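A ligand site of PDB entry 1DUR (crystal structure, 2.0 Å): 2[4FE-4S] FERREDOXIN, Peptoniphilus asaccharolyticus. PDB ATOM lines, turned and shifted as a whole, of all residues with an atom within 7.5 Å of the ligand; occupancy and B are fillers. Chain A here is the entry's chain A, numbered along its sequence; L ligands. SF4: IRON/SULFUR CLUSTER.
Ile 4 touches the ligand.
Ala 10 touches the ligand (CA to S3, 3.9 Å).
CB of Ala 13 touches S1 of the ligand, at 3.9 Å.
Tyr 29 touches the ligand.
Pro 47 touches the ligand (CD to S1, 3.97 Å).
Val 48 touches the ligand (CG2 to S4, 3.6 Å).
CB of Ala 50 touches S2 of the ligand (3.9 Å).
Pro 51 touches the ligand (CG to S2, 3.7 Å).
Hydrophobic or aromatic side chains within 4 Å of the ligand: Ile 4, Ile 9, Ala 13, Tyr 29, Pro 47, Val 48, Ala 50 and Pro 51.
Of the 30 residues printed, 14 come within 4 Å of the ligand.
The nearest printed residue that does not touch the ligand is Val 45 (4.8 Å).
The backbone NH of Cys 14 sits close to a sulfur (S1) of the ligand (3.5 Å).
FE4 of the ligand is bound by SG of Cys 14, at 2.2 Å.
A sulfur (S3) of the ligand sits close to the backbone NH (N) of Cys 11 (3.6 Å).
A sulfur (S4) of the ligand sits close to the backbone NH of Ile 9 (3.4 Å).
An iron atom (FE3) of the ligand is bound by the side-chain sulfur (SG) of Cys 46.
The side-chain sulfur (SG) of Cys 11 binds an iron atom (FE2) of the ligand (2.2 Å).
The side-chain sulfur of Cys 8 binds an iron atom (FE1) of the ligand (2.3 Å).
A sulfur (S3) of the ligand sits close to the backbone NH (N) of Gly 12, at 3.3 Å.
The side-chain sulfur (SG) of Cys 46 lies close to the backbone NH (N) of Ala 50, 3.4 Å away.
The side-chain sulfur (SG) of Cys 8 sits close to the backbone NH (N) of Ala 10, at 3.4 Å.
The side-chain sulfur (SG) of Cys 11 sits close to the backbone NH (N) of Ala 13 (3.5 Å).
SG of Cys 8 sits close to N of Tyr 29 (3.4 Å).
The side-chain sulfur (SG) of Cys 46 lies close to the backbone NH (N) of Gly 49 (3.5 Å).
SG of Cys 46 lies close to N of Val 48.
The backbone carbonyl oxygen of Ala 50 is in hydrogen-bond range of the backbone NH of Asn 5, at 2.9 Å.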
ATOM      1  N   VAL A   3      14.719  -0.671   8.178  1.00  0.00           N
ATOM      2  CA  VAL A   3      15.346   0.644   8.172  1.00  0.00           C
ATOM      3  C   VAL A   3      14.698   1.492   9.268  1.00  0.00           C
ATOM      4  O   VAL A   3      13.490   1.378   9.521  1.00  0.00           O
ATOM      5  CB  VAL A   3      15.222   1.346   6.795  1.00  0.00           C
ATOM      6  CG1 VAL A   3      13.773   1.469   6.385  1.00  0.00           C
ATOM      7  CG2 VAL A   3      15.887   2.713   6.829  1.00  0.00           C
ATOM      8  N   ILE A   4      15.496   2.263   9.984  1.00  0.00           N
ATOM      9  CA  ILE A   4      14.982   3.139  11.051  1.00  0.00           C
ATOM     10  C   ILE A   4      14.732   4.508  10.383  1.00  0.00           C
ATOM     11  O   ILE A   4      15.658   5.139   9.859  1.00  0.00           O
ATOM     12  CB  ILE A   4      15.993   3.227  12.236  1.00  0.00           C
ATOM     13  CG1 ILE A   4      16.042   1.859  12.967  1.00  0.00           C
ATOM     14  CG2 ILE A   4      15.617   4.319  13.201  1.00  0.00           C
ATOM     15  CD1 ILE A   4      17.023   1.785  14.122  1.00  0.00           C
ATOM     16  N   ASN A   5      13.454   4.891  10.330  1.00  0.00           N
ATOM     17  CA  ASN A   5      13.079   6.141   9.692  1.00  0.00           C
ATOM     18  C   ASN A   5      13.293   7.412  10.559  1.00  0.00           C
ATOM     19  O   ASN A   5      13.804   7.328  11.682  1.00  0.00           O
ATOM     20  CB  ASN A   5      11.679   6.051   9.062  1.00  0.00           C
ATOM     21  CG  ASN A   5      10.542   6.046  10.058  1.00  0.00           C
ATOM     22  OD1 ASN A   5      10.625   6.728  11.089  1.00  0.00           O
ATOM     23  ND2 ASN A   5       9.551   5.213   9.855  1.00  0.00           N
ATOM     24  N   SER A   7      11.463   9.163  12.361  1.00  0.00           N
ATOM     25  CA  SER A   7      10.749   9.217  13.636  1.00  0.00           C
ATOM     26  C   SER A   7      11.621   8.931  14.857  1.00  0.00           C
ATOM     27  O   SER A   7      11.294   9.295  15.980  1.00  0.00           O
ATOM     28  CB  SER A   7       9.605   8.209  13.656  1.00  0.00           C
ATOM     29  OG  SER A   7       8.506   8.671  12.907  1.00  0.00           O
ATOM     30  N   CYS A   8      12.714   8.218  14.609  1.00  0.00           N
ATOM     31  CA  CYS A   8      13.609   7.837  15.688  1.00  0.00           C
ATOM     32  C   CYS A   8      13.932   8.976  16.651  1.00  0.00           C
ATOM     33  O   CYS A   8      14.414  10.025  16.232  1.00  0.00           O
ATOM     34  CB  CYS A   8      14.883   7.226  15.116  1.00  0.00           C
ATOM     35  SG  CYS A   8      15.980   6.586  16.420  1.00  0.00           S
ATOM     36  N   ILE A   9      13.710   8.722  17.930  1.00  0.00           N
ATOM     37  CA  ILE A   9      13.992   9.698  18.990  1.00  0.00           C
ATOM     38  C   ILE A   9      15.200   9.296  19.817  1.00  0.00           C
ATOM     39  O   ILE A   9      15.398   9.851  20.909  1.00  0.00           O
ATOM     40  CB  ILE A   9      12.773   9.923  19.929  1.00  0.00           C
ATOM     41  CG1 ILE A   9      12.437   8.650  20.727  1.00  0.00           C
ATOM     42  CG2 ILE A   9      11.566  10.423  19.118  1.00  0.00           C
ATOM     43  CD1 ILE A   9      11.449   8.857  21.856  1.00  0.00           C
ATOM     44  N   ALA A  10      15.998   8.345  19.316  1.00  0.00           N
ATOM     45  CA  ALA A  10      17.228   7.849  19.936  1.00  0.00           C
ATOM     46  C   ALA A  10      17.131   7.405  21.394  1.00  0.00           C
ATOM     47  O   ALA A  10      18.030   7.661  22.204  1.00  0.00           O
ATOM     48  CB  ALA A  10      18.367   8.848  19.765  1.00  0.00           C
ATOM     49  N   CYS A  11      16.058   6.696  21.717  1.00  0.00           N
ATOM     50  CA  CYS A  11      15.856   6.203  23.077  1.00  0.00           C
ATOM     51  C   CYS A  11      16.823   5.056  23.428  1.00  0.00           C
ATOM     52  O   CYS A  11      17.267   4.949  24.571  1.00  0.00           O
ATOM     53  CB  CYS A  11      14.406   5.738  23.253  1.00  0.00           C
ATOM     54  SG  CYS A  11      13.943   4.334  22.206  1.00  0.00           S
ATOM     55  N   GLY A  12      17.172   4.241  22.435  1.00  0.00           N
ATOM     56  CA  GLY A  12      18.068   3.123  22.663  1.00  0.00           C
ATOM     57  C   GLY A  12      17.403   1.785  22.973  1.00  0.00           C
ATOM     58  O   GLY A  12      18.092   0.787  23.169  1.00  0.00           O
ATOM     59  N   ALA A  13      16.074   1.726  22.979  1.00  0.00           N
ATOM     60  CA  ALA A  13      15.356   0.489  23.288  1.00  0.00           C
ATOM     61  C   ALA A  13      15.604  -0.680  22.346  1.00  0.00           C
ATOM     62  O   ALA A  13      15.707  -1.819  22.778  1.00  0.00           O
ATOM     63  CB  ALA A  13      13.864   0.784  23.366  1.00  0.00           C
ATOM     64  N   CYS A  14      15.711  -0.388  21.051  1.00  0.00           N
ATOM     65  CA  CYS A  14      15.888  -1.423  20.039  1.00  0.00           C
ATOM     66  C   CYS A  14      17.206  -2.187  20.028  1.00  0.00           C
ATOM     67  O   CYS A  14      17.243  -3.379  19.738  1.00  0.00           O
ATOM     68  CB  CYS A  14      15.638  -0.795  18.668  1.00  0.00           C
ATOM     69  SG  CYS A  14      16.755   0.636  18.376  1.00  0.00           S
ATOM     70  N   LYS A  15      18.302  -1.507  20.352  1.00  0.00           N
ATOM     71  CA  LYS A  15      19.621  -2.138  20.314  1.00  0.00           C
ATOM     72  C   LYS A  15      19.764  -3.421  21.148  1.00  0.00           C
ATOM     73  O   LYS A  15      20.218  -4.447  20.624  1.00  0.00           O
ATOM     74  CB  LYS A  15      20.710  -1.114  20.697  1.00  0.00           C
ATOM     75  CG  LYS A  15      21.999  -1.317  19.935  1.00  0.00           C
ATOM     76  CD  LYS A  15      23.054  -0.275  20.266  1.00  0.00           C
ATOM     77  CE  LYS A  15      24.358  -0.967  20.614  1.00  0.00           C
ATOM     78  NZ  LYS A  15      24.988  -1.608  19.440  1.00  0.00           N
ATOM     79  N   ILE A  23      22.308  -3.149  15.146  1.00  0.00           N
ATOM     80  CA  ILE A  23      21.817  -1.767  15.266  1.00  0.00           C
ATOM     81  C   ILE A  23      22.922  -0.920  15.898  1.00  0.00           C
ATOM     82  O   ILE A  23      23.573  -1.363  16.850  1.00  0.00           O
ATOM     83  CB  ILE A  23      20.526  -1.646  16.110  1.00  0.00           C
ATOM     84  CG1 ILE A  23      19.365  -2.313  15.348  1.00  0.00           C
ATOM     85  CG2 ILE A  23      20.188  -0.190  16.402  1.00  0.00           C
ATOM     86  CD1 ILE A  23      18.053  -2.407  16.142  1.00  0.00           C
ATOM     87  N   GLN A  24      23.171   0.216  15.270  1.00  0.00           N
ATOM     88  CA  GLN A  24      24.181   1.181  15.712  1.00  0.00           C
ATOM     89  C   GLN A  24      23.491   2.474  16.137  1.00  0.00           C
ATOM     90  O   GLN A  24      22.504   2.910  15.560  1.00  0.00           O
ATOM     91  CB  GLN A  24      25.185   1.485  14.594  1.00  0.00           C
ATOM     92  CG  GLN A  24      25.936   0.274  14.044  1.00  0.00           C
ATOM     93  CD  GLN A  24      26.962  -0.316  15.003  1.00  0.00           C
ATOM     94  OE1 GLN A  24      27.353  -1.464  14.876  1.00  0.00           O
ATOM     95  NE2 GLN A  24      27.427   0.489  15.952  1.00  0.00           N
ATOM     96  N   GLU A  25      24.034   3.044  17.202  1.00  0.00           N
ATOM     97  CA  GLU A  25      23.598   4.292  17.787  1.00  0.00           C
ATOM     98  C   GLU A  25      24.069   5.455  16.909  1.00  0.00           C
ATOM     99  O   GLU A  25      25.105   5.372  16.266  1.00  0.00           O
ATOM    100  CB  GLU A  25      24.190   4.403  19.206  1.00  0.00           C
ATOM    101  CG  GLU A  25      25.690   3.988  19.355  1.00  0.00           C
ATOM    102  CD  GLU A  25      25.918   2.464  19.454  1.00  0.00           C
ATOM    103  OE1 GLU A  25      25.682   1.915  20.573  1.00  0.00           O
ATOM    104  OE2 GLU A  25      26.356   1.829  18.440  1.00  0.00           O
ATOM    105  N   GLY A  26      23.265   6.506  16.860  1.00  0.00           N
ATOM    106  CA  GLY A  26      23.573   7.696  16.097  1.00  0.00           C
ATOM    107  C   GLY A  26      22.549   8.773  16.444  1.00  0.00           C
ATOM    108  O   GLY A  26      21.731   8.530  17.334  1.00  0.00           O
ATOM    109  N   SER A  27      22.596   9.930  15.764  1.00  0.00           N
ATOM    110  CA  SER A  27      21.605  11.006  16.022  1.00  0.00           C
ATOM    111  C   SER A  27      20.237  10.317  15.936  1.00  0.00           C
ATOM    112  O   SER A  27      19.316  10.614  16.693  1.00  0.00           O
ATOM    113  CB  SER A  27      21.753  12.111  14.978  1.00  0.00           C
ATOM    114  N   ILE A  28      20.106   9.450  14.939  1.00  0.00           N
ATOM    115  CA  ILE A  28      18.962   8.558  14.834  1.00  0.00           C
ATOM    116  C   ILE A  28      19.695   7.196  14.691  1.00  0.00           C
ATOM    117  O   ILE A  28      20.794   7.139  14.124  1.00  0.00           O
ATOM    118  CB  ILE A  28      18.032   8.819  13.629  1.00  0.00           C
ATOM    119  CG1 ILE A  28      18.797   8.785  12.306  1.00  0.00           C
ATOM    120  CG2 ILE A  28      17.233  10.115  13.838  1.00  0.00           C
ATOM    121  CD1 ILE A  28      17.893   8.487  11.150  1.00  0.00           C
ATOM    122  N   TYR A  29      19.164   6.151  15.315  1.00  0.00           N
ATOM    123  CA  TYR A  29      19.815   4.842  15.230  1.00  0.00           C
ATOM    124  C   TYR A  29      19.778   4.305  13.803  1.00  0.00           C
ATOM    125  O   TYR A  29      18.946   4.718  13.008  1.00  0.00           O
ATOM    126  CB  TYR A  29      19.173   3.842  16.202  1.00  0.00           C
ATOM    127  CG  TYR A  29      19.648   4.033  17.624  1.00  0.00           C
ATOM    128  CD1 TYR A  29      19.734   5.294  18.203  1.00  0.00           C
ATOM    129  CD2 TYR A  29      20.060   2.930  18.375  1.00  0.00           C
ATOM    130  CE1 TYR A  29      20.224   5.463  19.493  1.00  0.00           C
ATOM    131  CE2 TYR A  29      20.547   3.080  19.649  1.00  0.00           C
ATOM    132  CZ  TYR A  29      20.636   4.343  20.212  1.00  0.00           C
ATOM    133  OH  TYR A  29      21.149   4.468  21.482  1.00  0.00           O
ATOM    134  N   ALA A  30      20.705   3.410  13.460  1.00  0.00           N
ATOM    135  CA  ALA A  30      20.765   2.891  12.113  1.00  0.00           C
ATOM    136  C   ALA A  30      21.038   1.392  12.088  1.00  0.00           C
ATOM    137  O   ALA A  30      21.803   0.886  12.898  1.00  0.00           O
ATOM    138  CB  ALA A  30      21.853   3.626  11.316  1.00  0.00           C
ATOM    139  N   ILE A  31      20.409   0.696  11.148  1.00  0.00           N
ATOM    140  CA  ILE A  31      20.560  -0.758  10.988  1.00  0.00           C
ATOM    141  C   ILE A  31      21.653  -1.152   9.957  1.00  0.00           C
ATOM    142  O   ILE A  31      21.784  -0.506   8.917  1.00  0.00           O
ATOM    143  CB  ILE A  31      19.197  -1.376  10.557  1.00  0.00           C
ATOM    144  CG1 ILE A  31      18.238  -1.403  11.756  1.00  0.00           C
ATOM    145  CG2 ILE A  31      19.369  -2.790   9.991  1.00  0.00           C
ATOM    146  CD1 ILE A  31      16.802  -1.638  11.371  1.00  0.00           C
ATOM    147  N   CYS A  42      12.958  -5.095  16.646  1.00  0.00           N
ATOM    148  CA  CYS A  42      13.178  -3.669  16.849  1.00  0.00           C
ATOM    149  C   CYS A  42      11.859  -2.921  16.655  1.00  0.00           C
ATOM    150  O   CYS A  42      11.509  -2.060  17.453  1.00  0.00           O
ATOM    151  CB  CYS A  42      14.239  -3.143  15.883  1.00  0.00           C
ATOM    152  SG  CYS A  42      13.981  -3.670  14.184  1.00  0.00           S
ATOM    153  N   ALA A  43      11.119  -3.294  15.619  1.00  0.00           N
ATOM    154  CA  ALA A  43       9.830  -2.671  15.335  1.00  0.00           C
ATOM    155  C   ALA A  43       8.899  -2.905  16.525  1.00  0.00           C
ATOM    156  O   ALA A  43       8.116  -2.046  16.890  1.00  0.00           O
ATOM    157  CB  ALA A  43       9.195  -3.253  14.090  1.00  0.00           C
ATOM    158  N   VAL A  45       9.569  -3.259  19.872  1.00  0.00           N
ATOM    159  CA  VAL A  45       9.823  -2.429  21.065  1.00  0.00           C
ATOM    160  C   VAL A  45       9.892  -0.906  20.861  1.00  0.00           C
ATOM    161  O   VAL A  45       9.965  -0.160  21.840  1.00  0.00           O
ATOM    162  CB  VAL A  45      11.170  -2.772  21.790  1.00  0.00           C
ATOM    163  CG1 VAL A  45      11.102  -4.153  22.425  1.00  0.00           C
ATOM    164  CG2 VAL A  45      12.342  -2.663  20.822  1.00  0.00           C
ATOM    165  N   CYS A  46       9.958  -0.452  19.619  1.00  0.00           N
ATOM    166  CA  CYS A  46      10.064   0.976  19.384  1.00  0.00           C
ATOM    167  C   CYS A  46       8.819   1.751  19.814  1.00  0.00           C
ATOM    168  O   CYS A  46       7.712   1.468  19.365  1.00  0.00           O
ATOM    169  CB  CYS A  46      10.413   1.272  17.927  1.00  0.00           C
ATOM    170  SG  CYS A  46      10.673   3.050  17.632  1.00  0.00           S
ATOM    171  N   PRO A  47       8.992   2.764  20.681  1.00  0.00           N
ATOM    172  CA  PRO A  47       7.863   3.561  21.137  1.00  0.00           C
ATOM    173  C   PRO A  47       7.268   4.475  20.054  1.00  0.00           C
ATOM    174  O   PRO A  47       6.127   4.902  20.201  1.00  0.00           O
ATOM    175  CB  PRO A  47       8.459   4.388  22.287  1.00  0.00           C
ATOM    176  CG  PRO A  47       9.896   4.513  21.931  1.00  0.00           C
ATOM    177  CD  PRO A  47      10.231   3.130  21.406  1.00  0.00           C
ATOM    178  N   VAL A  48       7.996   4.709  18.968  1.00  0.00           N
ATOM    179  CA  VAL A  48       7.509   5.622  17.929  1.00  0.00           C
ATOM    180  C   VAL A  48       7.343   4.991  16.535  1.00  0.00           C
ATOM    181  O   VAL A  48       7.092   5.708  15.558  1.00  0.00           O
ATOM    182  CB  VAL A  48       8.388   6.920  17.833  1.00  0.00           C
ATOM    183  CG1 VAL A  48       8.183   7.784  19.057  1.00  0.00           C
ATOM    184  CG2 VAL A  48       9.877   6.580  17.753  1.00  0.00           C
ATOM    185  N   GLY A  49       7.469   3.675  16.468  1.00  0.00           N
ATOM    186  CA  GLY A  49       7.345   2.958  15.193  1.00  0.00           C
ATOM    187  C   GLY A  49       8.307   3.362  14.094  1.00  0.00           C
ATOM    188  O   GLY A  49       7.917   3.403  12.933  1.00  0.00           O
ATOM    189  N   ALA A  50       9.544   3.637  14.442  1.00  0.00           N
ATOM    190  CA  ALA A  50      10.562   4.044  13.462  1.00  0.00           C
ATOM    191  C   ALA A  50      11.116   2.914  12.560  1.00  0.00           C
ATOM    192  O   ALA A  50      11.392   3.161  11.378  1.00  0.00           O
ATOM    193  CB  ALA A  50      11.726   4.793  14.166  1.00  0.00           C
ATOM    194  N   PRO A  51      11.347   1.699  13.111  1.00  0.00           N
ATOM    195  CA  PRO A  51      11.887   0.592  12.341  1.00  0.00           C
ATOM    196  C   PRO A  51      10.807  -0.023  11.483  1.00  0.00           C
ATOM    197  O   PRO A  51       9.773  -0.453  12.023  1.00  0.00           O
ATOM    198  CB  PRO A  51      12.358  -0.403  13.394  1.00  0.00           C
ATOM    199  CG  PRO A  51      12.441   0.397  14.657  1.00  0.00           C
ATOM    200  CD  PRO A  51      11.221   1.278  14.526  1.00  0.00           C
HETATM  201 FE1  SF4 L   1      14.963   4.882  17.586  1.00  0.00          FE
HETATM  202 FE2  SF4 L   1      14.239   4.104  20.069  1.00  0.00          FE
HETATM  203 FE3  SF4 L   1      12.798   3.313  18.111  1.00  0.00          FE
HETATM  204 FE4  SF4 L   1      15.314   2.352  18.314  1.00  0.00          FE
HETATM  205  S1  SF4 L   1      13.622   2.007  19.664  1.00  0.00           S
HETATM  206  S2  SF4 L   1      14.322   3.068  16.460  1.00  0.00           S
HETATM  207  S3  SF4 L   1      16.283   4.093  19.218  1.00  0.00           S
HETATM  208  S4  SF4 L   1      13.143   5.435  18.736  1.00  0.00           S
